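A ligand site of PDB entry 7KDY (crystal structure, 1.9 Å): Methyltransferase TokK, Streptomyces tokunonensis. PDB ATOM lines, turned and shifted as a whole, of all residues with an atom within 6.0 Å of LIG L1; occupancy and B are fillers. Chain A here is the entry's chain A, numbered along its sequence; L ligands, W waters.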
ATOM      1  N   CYS A 206      -7.970 -17.273 -21.142  1.00  0.00           N
ATOM      2  CA  CYS A 206      -7.108 -17.693 -20.057  1.00  0.00           C
ATOM      3  C   CYS A 206      -7.838 -17.346 -18.760  1.00  0.00           C
ATOM      4  O   CYS A 206      -8.332 -16.217 -18.615  1.00  0.00           O
ATOM      5  CB  CYS A 206      -5.739 -17.028 -20.082  1.00  0.00           C
ATOM      6  SG  CYS A 206      -4.838 -17.457 -18.574  1.00  0.00           S
ATOM      7  N   TYR A 208      -6.634 -16.780 -15.865  1.00  0.00           N
ATOM      8  CA  TYR A 208      -5.774 -16.079 -14.919  1.00  0.00           C
ATOM      9  C   TYR A 208      -5.721 -14.582 -15.266  1.00  0.00           C
ATOM     10  O   TYR A 208      -6.451 -14.109 -16.141  1.00  0.00           O
ATOM     11  CB  TYR A 208      -4.418 -16.766 -14.874  1.00  0.00           C
ATOM     12  CG  TYR A 208      -4.583 -18.255 -14.654  1.00  0.00           C
ATOM     13  CD1 TYR A 208      -5.171 -18.745 -13.482  1.00  0.00           C
ATOM     14  CD2 TYR A 208      -4.196 -19.175 -15.615  1.00  0.00           C
ATOM     15  CE1 TYR A 208      -5.347 -20.101 -13.272  1.00  0.00           C
ATOM     16  CE2 TYR A 208      -4.370 -20.543 -15.420  1.00  0.00           C
ATOM     17  CZ  TYR A 208      -4.939 -20.993 -14.253  1.00  0.00           C
ATOM     18  OH  TYR A 208      -5.111 -22.344 -14.073  1.00  0.00           O
ATOM     19  N   CYS A 210      -2.594 -12.221 -15.168  1.00  0.00           N
ATOM     20  CA  CYS A 210      -1.301 -11.545 -15.199  1.00  0.00           C
ATOM     21  C   CYS A 210      -1.416 -10.179 -15.895  1.00  0.00           C
ATOM     22  O   CYS A 210      -1.872 -10.099 -17.031  1.00  0.00           O
ATOM     23  CB  CYS A 210      -0.264 -12.421 -15.897  1.00  0.00           C
ATOM     24  SG  CYS A 210      -0.156 -14.046 -15.140  1.00  0.00           S
ATOM     25  N   CYS A 213      -0.245  -9.197 -19.539  1.00  0.00           N
ATOM     26  CA  CYS A 213      -0.643 -10.072 -20.630  1.00  0.00           C
ATOM     27  C   CYS A 213      -1.969  -9.650 -21.252  1.00  0.00           C
ATOM     28  O   CYS A 213      -2.825  -9.057 -20.606  1.00  0.00           O
ATOM     29  CB  CYS A 213      -0.749 -11.519 -20.134  1.00  0.00           C
ATOM     30  SG  CYS A 213      -0.937 -12.723 -21.445  1.00  0.00           S
ATOM     31  N   TRP A 215      -3.448 -12.163 -23.630  1.00  0.00           N
ATOM     32  CA  TRP A 215      -3.530 -13.384 -24.421  1.00  0.00           C
ATOM     33  C   TRP A 215      -4.901 -13.544 -25.080  1.00  0.00           C
ATOM     34  O   TRP A 215      -5.918 -13.692 -24.391  1.00  0.00           O
ATOM     35  CB  TRP A 215      -3.242 -14.594 -23.533  1.00  0.00           C
ATOM     36  CG  TRP A 215      -2.771 -15.778 -24.307  1.00  0.00           C
ATOM     37  CD1 TRP A 215      -3.508 -16.840 -24.743  1.00  0.00           C
ATOM     38  CD2 TRP A 215      -1.428 -16.011 -24.772  1.00  0.00           C
ATOM     39  NE1 TRP A 215      -2.722 -17.729 -25.423  1.00  0.00           N
ATOM     40  CE2 TRP A 215      -1.434 -17.246 -25.463  1.00  0.00           C
ATOM     41  CE3 TRP A 215      -0.236 -15.299 -24.663  1.00  0.00           C
ATOM     42  CZ2 TRP A 215      -0.284 -17.772 -26.047  1.00  0.00           C
ATOM     43  CZ3 TRP A 215       0.906 -15.822 -25.252  1.00  0.00           C
ATOM     44  CH2 TRP A 215       0.870 -17.050 -25.926  1.00  0.00           C
ATOM     45  N   ASP A 250      -3.443 -21.959 -27.671  1.00  0.00           N
ATOM     46  CA  ASP A 250      -4.027 -22.050 -26.336  1.00  0.00           C
ATOM     47  C   ASP A 250      -3.119 -21.399 -25.288  1.00  0.00           C
ATOM     48  O   ASP A 250      -1.894 -21.455 -25.364  1.00  0.00           O
ATOM     49  CB  ASP A 250      -4.270 -23.506 -25.956  1.00  0.00           C
ATOM     50  CG  ASP A 250      -5.312 -24.185 -26.827  1.00  0.00           C
ATOM     51  OD1 ASP A 250      -5.750 -23.599 -27.839  1.00  0.00           O
ATOM     52  OD2 ASP A 250      -5.675 -25.336 -26.501  1.00  0.00           O
ATOM     53  N   ALA A 251      -3.756 -20.793 -24.278  1.00  0.00           N
ATOM     54  CA  ALA A 251      -3.001 -20.166 -23.204  1.00  0.00           C
ATOM     55  C   ALA A 251      -2.426 -21.182 -22.230  1.00  0.00           C
ATOM     56  O   ALA A 251      -1.331 -20.971 -21.692  1.00  0.00           O
ATOM     57  CB  ALA A 251      -3.892 -19.182 -22.447  1.00  0.00           C
ATOM     58  N   ASN A 252      -3.138 -22.303 -21.990  1.00  0.00           N
ATOM     59  CA  ASN A 252      -2.794 -23.243 -20.940  1.00  0.00           C
ATOM     60  C   ASN A 252      -3.035 -24.683 -21.421  1.00  0.00           C
ATOM     61  O   ASN A 252      -3.918 -25.383 -20.916  1.00  0.00           O
ATOM     62  CB  ASN A 252      -3.615 -22.981 -19.675  1.00  0.00           C
ATOM     63  CG  ASN A 252      -3.284 -21.653 -19.033  1.00  0.00           C
ATOM     64  OD1 ASN A 252      -2.275 -21.526 -18.343  1.00  0.00           O
ATOM     65  ND2 ASN A 252      -4.133 -20.649 -19.267  1.00  0.00           N
ATOM     66  N   ASN A 282       1.860 -23.291 -25.651  1.00  0.00           N
ATOM     67  CA  ASN A 282       2.125 -22.876 -24.290  1.00  0.00           C
ATOM     68  C   ASN A 282       1.361 -23.789 -23.334  1.00  0.00           C
ATOM     69  O   ASN A 282       0.136 -23.905 -23.429  1.00  0.00           O
ATOM     70  CB  ASN A 282       1.709 -21.423 -24.081  1.00  0.00           C
ATOM     71  CG  ASN A 282       2.685 -20.455 -24.723  1.00  0.00           C
ATOM     72  OD1 ASN A 282       3.680 -20.077 -24.105  1.00  0.00           O
ATOM     73  ND2 ASN A 282       2.409 -20.060 -25.959  1.00  0.00           N
ATOM     74  N   PHE A 283       2.083 -24.428 -22.412  1.00  0.00           N
ATOM     75  CA  PHE A 283       1.485 -25.368 -21.477  1.00  0.00           C
ATOM     76  C   PHE A 283       1.015 -24.653 -20.207  1.00  0.00           C
ATOM     77  O   PHE A 283       1.485 -23.565 -19.858  1.00  0.00           O
ATOM     78  CB  PHE A 283       2.484 -26.478 -21.132  1.00  0.00           C
ATOM     79  CG  PHE A 283       2.689 -27.476 -22.248  1.00  0.00           C
ATOM     80  CD1 PHE A 283       3.673 -27.267 -23.206  1.00  0.00           C
ATOM     81  CD2 PHE A 283       1.918 -28.624 -22.323  1.00  0.00           C
ATOM     82  CE1 PHE A 283       3.875 -28.190 -24.228  1.00  0.00           C
ATOM     83  CE2 PHE A 283       2.115 -29.554 -23.340  1.00  0.00           C
ATOM     84  CZ  PHE A 283       3.097 -29.339 -24.290  1.00  0.00           C
ATOM     85  N   ALA A 284       0.094 -25.313 -19.491  1.00  0.00           N
ATOM     86  CA  ALA A 284      -0.676 -24.681 -18.429  1.00  0.00           C
ATOM     87  C   ALA A 284       0.203 -24.132 -17.310  1.00  0.00           C
ATOM     88  O   ALA A 284       1.210 -24.724 -16.932  1.00  0.00           O
ATOM     89  CB  ALA A 284      -1.670 -25.683 -17.852  1.00  0.00           C
ATOM     90  N   LYS A 285      -0.207 -22.968 -16.775  1.00  0.00           N
ATOM     91  CA  LYS A 285       0.521 -22.344 -15.674  1.00  0.00           C
ATOM     92  C   LYS A 285       0.585 -23.255 -14.463  1.00  0.00           C
ATOM     93  O   LYS A 285       1.658 -23.488 -13.893  1.00  0.00           O
ATOM     94  CB  LYS A 285      -0.122 -21.015 -15.299  1.00  0.00           C
ATOM     95  CG  LYS A 285       0.629 -20.271 -14.192  1.00  0.00           C
ATOM     96  CD  LYS A 285       0.145 -18.844 -14.011  1.00  0.00           C
ATOM     97  CE  LYS A 285      -1.273 -18.816 -13.446  1.00  0.00           C
ATOM     98  NZ  LYS A 285      -1.322 -19.430 -12.094  1.00  0.00           N
ATOM     99  N   ASN A 286      -0.573 -23.775 -14.044  1.00  0.00           N
ATOM    100  CA  ASN A 286      -0.633 -24.712 -12.919  1.00  0.00           C
ATOM    101  C   ASN A 286      -0.350 -26.106 -13.461  1.00  0.00           C
ATOM    102  O   ASN A 286      -1.235 -26.955 -13.609  1.00  0.00           O
ATOM    103  CB  ASN A 286      -1.989 -24.632 -12.219  1.00  0.00           C
ATOM    104  CG  ASN A 286      -2.295 -23.241 -11.704  1.00  0.00           C
ATOM    105  OD1 ASN A 286      -1.400 -22.408 -11.567  1.00  0.00           O
ATOM    106  ND2 ASN A 286      -3.564 -22.980 -11.439  1.00  0.00           N
ATOM    107  N   THR A 308       6.226 -25.857 -21.141  1.00  0.00           N
ATOM    108  CA  THR A 308       6.265 -24.537 -20.518  1.00  0.00           C
ATOM    109  C   THR A 308       6.112 -24.671 -19.009  1.00  0.00           C
ATOM    110  O   THR A 308       5.089 -25.157 -18.521  1.00  0.00           O
ATOM    111  CB  THR A 308       5.159 -23.647 -21.073  1.00  0.00           C
ATOM    112  OG1 THR A 308       5.010 -23.888 -22.475  1.00  0.00           O
ATOM    113  CG2 THR A 308       5.506 -22.177 -20.855  1.00  0.00           C
ATOM    114  N   LEU A 309       7.135 -24.226 -18.272  1.00  0.00           N
ATOM    115  CA  LEU A 309       7.062 -24.075 -16.810  1.00  0.00           C
ATOM    116  C   LEU A 309       7.521 -22.646 -16.489  1.00  0.00           C
ATOM    117  O   LEU A 309       8.570 -22.440 -15.887  1.00  0.00           O
ATOM    118  CB  LEU A 309       7.923 -25.112 -16.096  1.00  0.00           C
ATOM    119  CG  LEU A 309       7.597 -26.585 -16.336  1.00  0.00           C
ATOM    120  CD1 LEU A 309       8.657 -27.474 -15.709  1.00  0.00           C
ATOM    121  CD2 LEU A 309       6.229 -26.908 -15.756  1.00  0.00           C
ATOM    122  N   SER A 310       6.730 -21.664 -16.907  1.00  0.00           N
ATOM    123  CA  SER A 310       7.171 -20.279 -16.881  1.00  0.00           C
ATOM    124  C   SER A 310       6.830 -19.600 -15.563  1.00  0.00           C
ATOM    125  O   SER A 310       5.911 -19.996 -14.847  1.00  0.00           O
ATOM    126  CB  SER A 310       6.582 -19.501 -18.050  1.00  0.00           C
ATOM    127  OG  SER A 310       7.250 -19.814 -19.266  1.00  0.00           O
ATOM    128  N   MET A 311       7.602 -18.565 -15.246  1.00  0.00           N
ATOM    129  CA  MET A 311       7.526 -17.900 -13.946  1.00  0.00           C
ATOM    130  C   MET A 311       7.292 -16.395 -14.089  1.00  0.00           C
ATOM    131  O   MET A 311       6.631 -15.792 -13.226  1.00  0.00           O
ATOM    132  CB  MET A 311       8.816 -18.154 -13.157  1.00  0.00           C
ATOM    133  CG  MET A 311       8.995 -19.590 -12.723  1.00  0.00           C
ATOM    134  SD  MET A 311       7.891 -19.937 -11.347  1.00  0.00           S
ATOM    135  CE  MET A 311       8.139 -21.679 -11.093  1.00  0.00           C
ATOM    136  N   GLN A 312       7.832 -15.798 -15.148  1.00  0.00           N
ATOM    137  CA  GLN A 312       7.885 -14.355 -15.370  1.00  0.00           C
ATOM    138  C   GLN A 312       8.780 -13.683 -14.327  1.00  0.00           C
ATOM    139  O   GLN A 312       9.689 -12.924 -14.668  1.00  0.00           O
ATOM    140  CB  GLN A 312       6.480 -13.728 -15.369  1.00  0.00           C
ATOM    141  CG  GLN A 312       5.375 -14.611 -15.968  1.00  0.00           C
ATOM    142  CD  GLN A 312       5.644 -15.056 -17.403  1.00  0.00           C
ATOM    143  OE1 GLN A 312       6.635 -14.657 -18.020  1.00  0.00           O
ATOM    144  NE2 GLN A 312       4.735 -15.855 -17.942  1.00  0.00           N
ATOM    145  N   ARG A 324      -0.030 -12.468 -10.307  1.00  0.00           N
ATOM    146  CA  ARG A 324       0.313 -13.815 -10.762  1.00  0.00           C
ATOM    147  C   ARG A 324       0.759 -14.656  -9.571  1.00  0.00           C
ATOM    148  O   ARG A 324       1.559 -14.198  -8.756  1.00  0.00           O
ATOM    149  CB  ARG A 324       1.409 -13.797 -11.819  1.00  0.00           C
ATOM    150  CG  ARG A 324       1.806 -15.193 -12.304  1.00  0.00           C
ATOM    151  CD  ARG A 324       2.917 -15.116 -13.343  1.00  0.00           C
ATOM    152  NE  ARG A 324       3.414 -16.438 -13.705  1.00  0.00           N
ATOM    153  CZ  ARG A 324       3.060 -17.100 -14.801  1.00  0.00           C
ATOM    154  NH1 ARG A 324       2.207 -16.566 -15.665  1.00  0.00           N
ATOM    155  NH2 ARG A 324       3.572 -18.300 -15.042  1.00  0.00           N
ATOM    156  N   ASN A 326       2.647 -18.247  -8.915  1.00  0.00           N
ATOM    157  CA  ASN A 326       3.422 -19.338  -9.503  1.00  0.00           C
ATOM    158  C   ASN A 326       3.344 -20.572  -8.617  1.00  0.00           C
ATOM    159  O   ASN A 326       2.973 -20.506  -7.440  1.00  0.00           O
ATOM    160  CB  ASN A 326       4.886 -18.935  -9.702  1.00  0.00           C
ATOM    161  CG  ASN A 326       5.092 -18.053 -10.905  1.00  0.00           C
ATOM    162  OD1 ASN A 326       4.439 -18.215 -11.940  1.00  0.00           O
ATOM    163  ND2 ASN A 326       6.033 -17.116 -10.798  1.00  0.00           N
ATOM    164  N   GLU A 349      10.202 -19.112 -18.830  1.00  0.00           N
ATOM    165  CA  GLU A 349      10.297 -17.738 -19.318  1.00  0.00           C
ATOM    166  C   GLU A 349      10.301 -16.750 -18.152  1.00  0.00           C
ATOM    167  O   GLU A 349       9.626 -16.955 -17.142  1.00  0.00           O
ATOM    168  CB  GLU A 349       9.137 -17.401 -20.254  1.00  0.00           C
ATOM    169  CG  GLU A 349       9.137 -18.226 -21.532  1.00  0.00           C
ATOM    170  CD  GLU A 349       7.766 -18.287 -22.156  1.00  0.00           C
ATOM    171  OE1 GLU A 349       6.782 -18.523 -21.414  1.00  0.00           O
ATOM    172  OE2 GLU A 349       7.673 -18.103 -23.385  1.00  0.00           O
HETATM  173  N1  LIG L   1      -0.256 -19.570 -19.332  1.00  0.00           N
HETATM  174  C1  LIG L   1       1.043 -20.196 -19.069  1.00  0.00           C
HETATM  175  C2  LIG L   1       1.834 -19.425 -18.020  1.00  0.00           C
HETATM  176  O1  LIG L   1       1.693 -18.212 -17.847  1.00  0.00           O
HETATM  177  C3  LIG L   1       1.850 -20.321 -20.360  1.00  0.00           C
HETATM  178  C4  LIG L   1       2.656 -19.090 -20.748  1.00  0.00           C
HETATM  179  S1  LIG L   1       1.655 -17.660 -21.182  1.00  0.00           S
HETATM  180  C5  LIG L   1       0.702 -18.306 -22.546  1.00  0.00           C
HETATM  181  O2  LIG L   1       2.658 -20.005 -17.306  1.00  0.00           O
HETATM  182 FE1  LG2 L   2      -0.764 -15.226 -17.270  1.00  0.00          FE
HETATM  183 FE2  LG2 L   2      -2.699 -16.383 -18.686  1.00  0.00          FE
HETATM  184 FE3  LG2 L   2      -0.079 -17.149 -19.103  1.00  0.00          FE
HETATM  185 FE4  LG2 L   2      -1.014 -14.673 -19.880  1.00  0.00          FE
HETATM  186  S1  LG2 L   2      -1.679 -16.656 -20.682  1.00  0.00           S
HETATM  187  S2  LG2 L   2       0.926 -15.118 -18.785  1.00  0.00           S
HETATM  188  S3  LG2 L   2      -2.508 -14.201 -18.251  1.00  0.00           S
HETATM  189  S4  LG2 L   2      -1.334 -17.370 -17.166  1.00  0.00           S
HETATM  190  N1  LG3 L   3       5.893  -8.480 -22.586  1.00  0.00           N
HETATM  191  C1  LG3 L   3       6.811  -9.448 -22.705  1.00  0.00           C
HETATM  192  N2  LG3 L   3       6.636 -10.772 -22.667  1.00  0.00           N
HETATM  193  C2  LG3 L   3       5.347 -11.094 -22.514  1.00  0.00           C
HETATM  194  N3  LG3 L   3       4.803 -12.348 -22.415  1.00  0.00           N
HETATM  195  C3  LG3 L   3       3.464 -12.163 -22.266  1.00  0.00           C
HETATM  196  N4  LG3 L   3       3.095 -10.895 -22.236  1.00  0.00           N
HETATM  197  C4  LG3 L   3       4.297 -10.212 -22.392  1.00  0.00           C
HETATM  198  C5  LG3 L   3       4.597  -8.832 -22.421  1.00  0.00           C
HETATM  199  N5  LG3 L   3       3.668  -7.892 -22.253  1.00  0.00           N
HETATM  200  C6  LG3 L   3       5.537 -13.612 -22.411  1.00  0.00           C
HETATM  201  C7  LG3 L   3       5.476 -14.362 -21.077  1.00  0.00           C
HETATM  202  C8  LG3 L   3       4.625 -15.592 -21.423  1.00  0.00           C
HETATM  203  C9  LG3 L   3       4.960 -15.804 -22.890  1.00  0.00           C
HETATM  204  C10 LG3 L   3       3.963 -16.618 -23.678  1.00  0.00           C
HETATM  205  O1  LG3 L   3       5.000 -14.459 -23.413  1.00  0.00           O
HETATM  206  O2  LG3 L   3       6.806 -14.724 -20.704  1.00  0.00           O
HETATM  207  O3  LG3 L   3       4.992 -16.748 -20.675  1.00  0.00           O
HETATM  208  O   HOH W   1       3.834 -22.382 -17.640  1.00  0.00           O
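An iron atom (FE3) of LG2 L2 is bound by an oxygen (O1) of LIG L1 (2.4 Å).
A sulfur (S1) of LIG L1 sits close to an oxygen (O3) of LG3 L3 (3.5 Å).
Water W1 lies within hydrogen-bond range of an oxygen (O2) of LIG L1 (2.7 Å), the backbone NH of Ser 310 (3.1 Å), the backbone carbonyl oxygen of Thr 308 (3.2 Å) and the backbone carbonyl oxygen of Phe 283 (3.4 Å).
The backbone carbonyl oxygen (O) of Glu 349 lies within hydrogen-bond range of the backbone NH (N) of Gln 312 (2.9 Å).
NE of Arg 324 sits at hydrogen-bond distance from O of Met 311, at 3.3 Å.
The side-chain amide oxygen (OD1) of Asn 252 sits at hydrogen-bond distance from the backbone NH (N) of Lys 285, 3.0 Å away.
NE2 of Gln 312 sits close to NH1 of Arg 324 (3.5 Å).
The side-chain amino group (NZ) of Lys 285 is in hydrogen-bond range of the side-chain amide oxygen (OD1) of Asn 286 (3.0 Å).
SG of Cys 206 lies close to ND2 of Asn 252 (3.3 Å).
The guanidinium group (NE) of Arg 324 sits at hydrogen-bond distance from the side-chain amide oxygen (OD1) of Asn 326, at 2.7 Å.
NH2 of Arg 324 is in hydrogen-bond range of O of Ser 310.
CH2 of Trp 215 touches C5 of LIG L1 (3.6 Å).
Asn 282 touches LIG L1 (CB to C5, 3.6 Å).
O of Phe 283 touches C3 of LIG L1, 3.3 Å away.
Lys 285 touches LIG L1.
Gln 312 touches LIG L1 (NE2 to O1, 3.8 Å).
Hydrophobic or aromatic side chains that line LIG L1: Trp 215.
Of the 21 residues printed, 8 come within 4 Å of LIG L1.
Along chain A the residues within 4 Å of LIG L1 span positions 215 to 324.
O of Ala 251 lies close to N1 of LIG L1 (2.9 Å).
SG of Cys 206 is bound to FE2 of LG2 L2 (2.4 Å).
A sulfur (S3) of LG2 L2 lies close to the backbone NH (N) of Cys 210, at 3.7 Å.
The side-chain sulfur (SG) of Cys 210 binds an iron atom (FE1) of LG2 L2 (2.5 Å).
The guanidinium group (NH2) of Arg 324 is in salt-bridge range of an oxygen (O2) of LIG L1, at 3.0 Å.
The side-chain carboxylate (OE1) of Glu 349 sits at hydrogen-bond distance from an oxygen (O3) of LG3 L3 (2.6 Å).
SG of Cys 213 binds FE4 of LG2 L2 (2.5 Å).
S2 of LG2 L2 lies close to NH1 of Arg 324 (3.7 Å).
An oxygen (O2) of LG3 L3 is in hydrogen-bond range of the side-chain amide oxygen of Gln 312.
N1 of LIG L1 sits close to OD1 of Asn 252.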
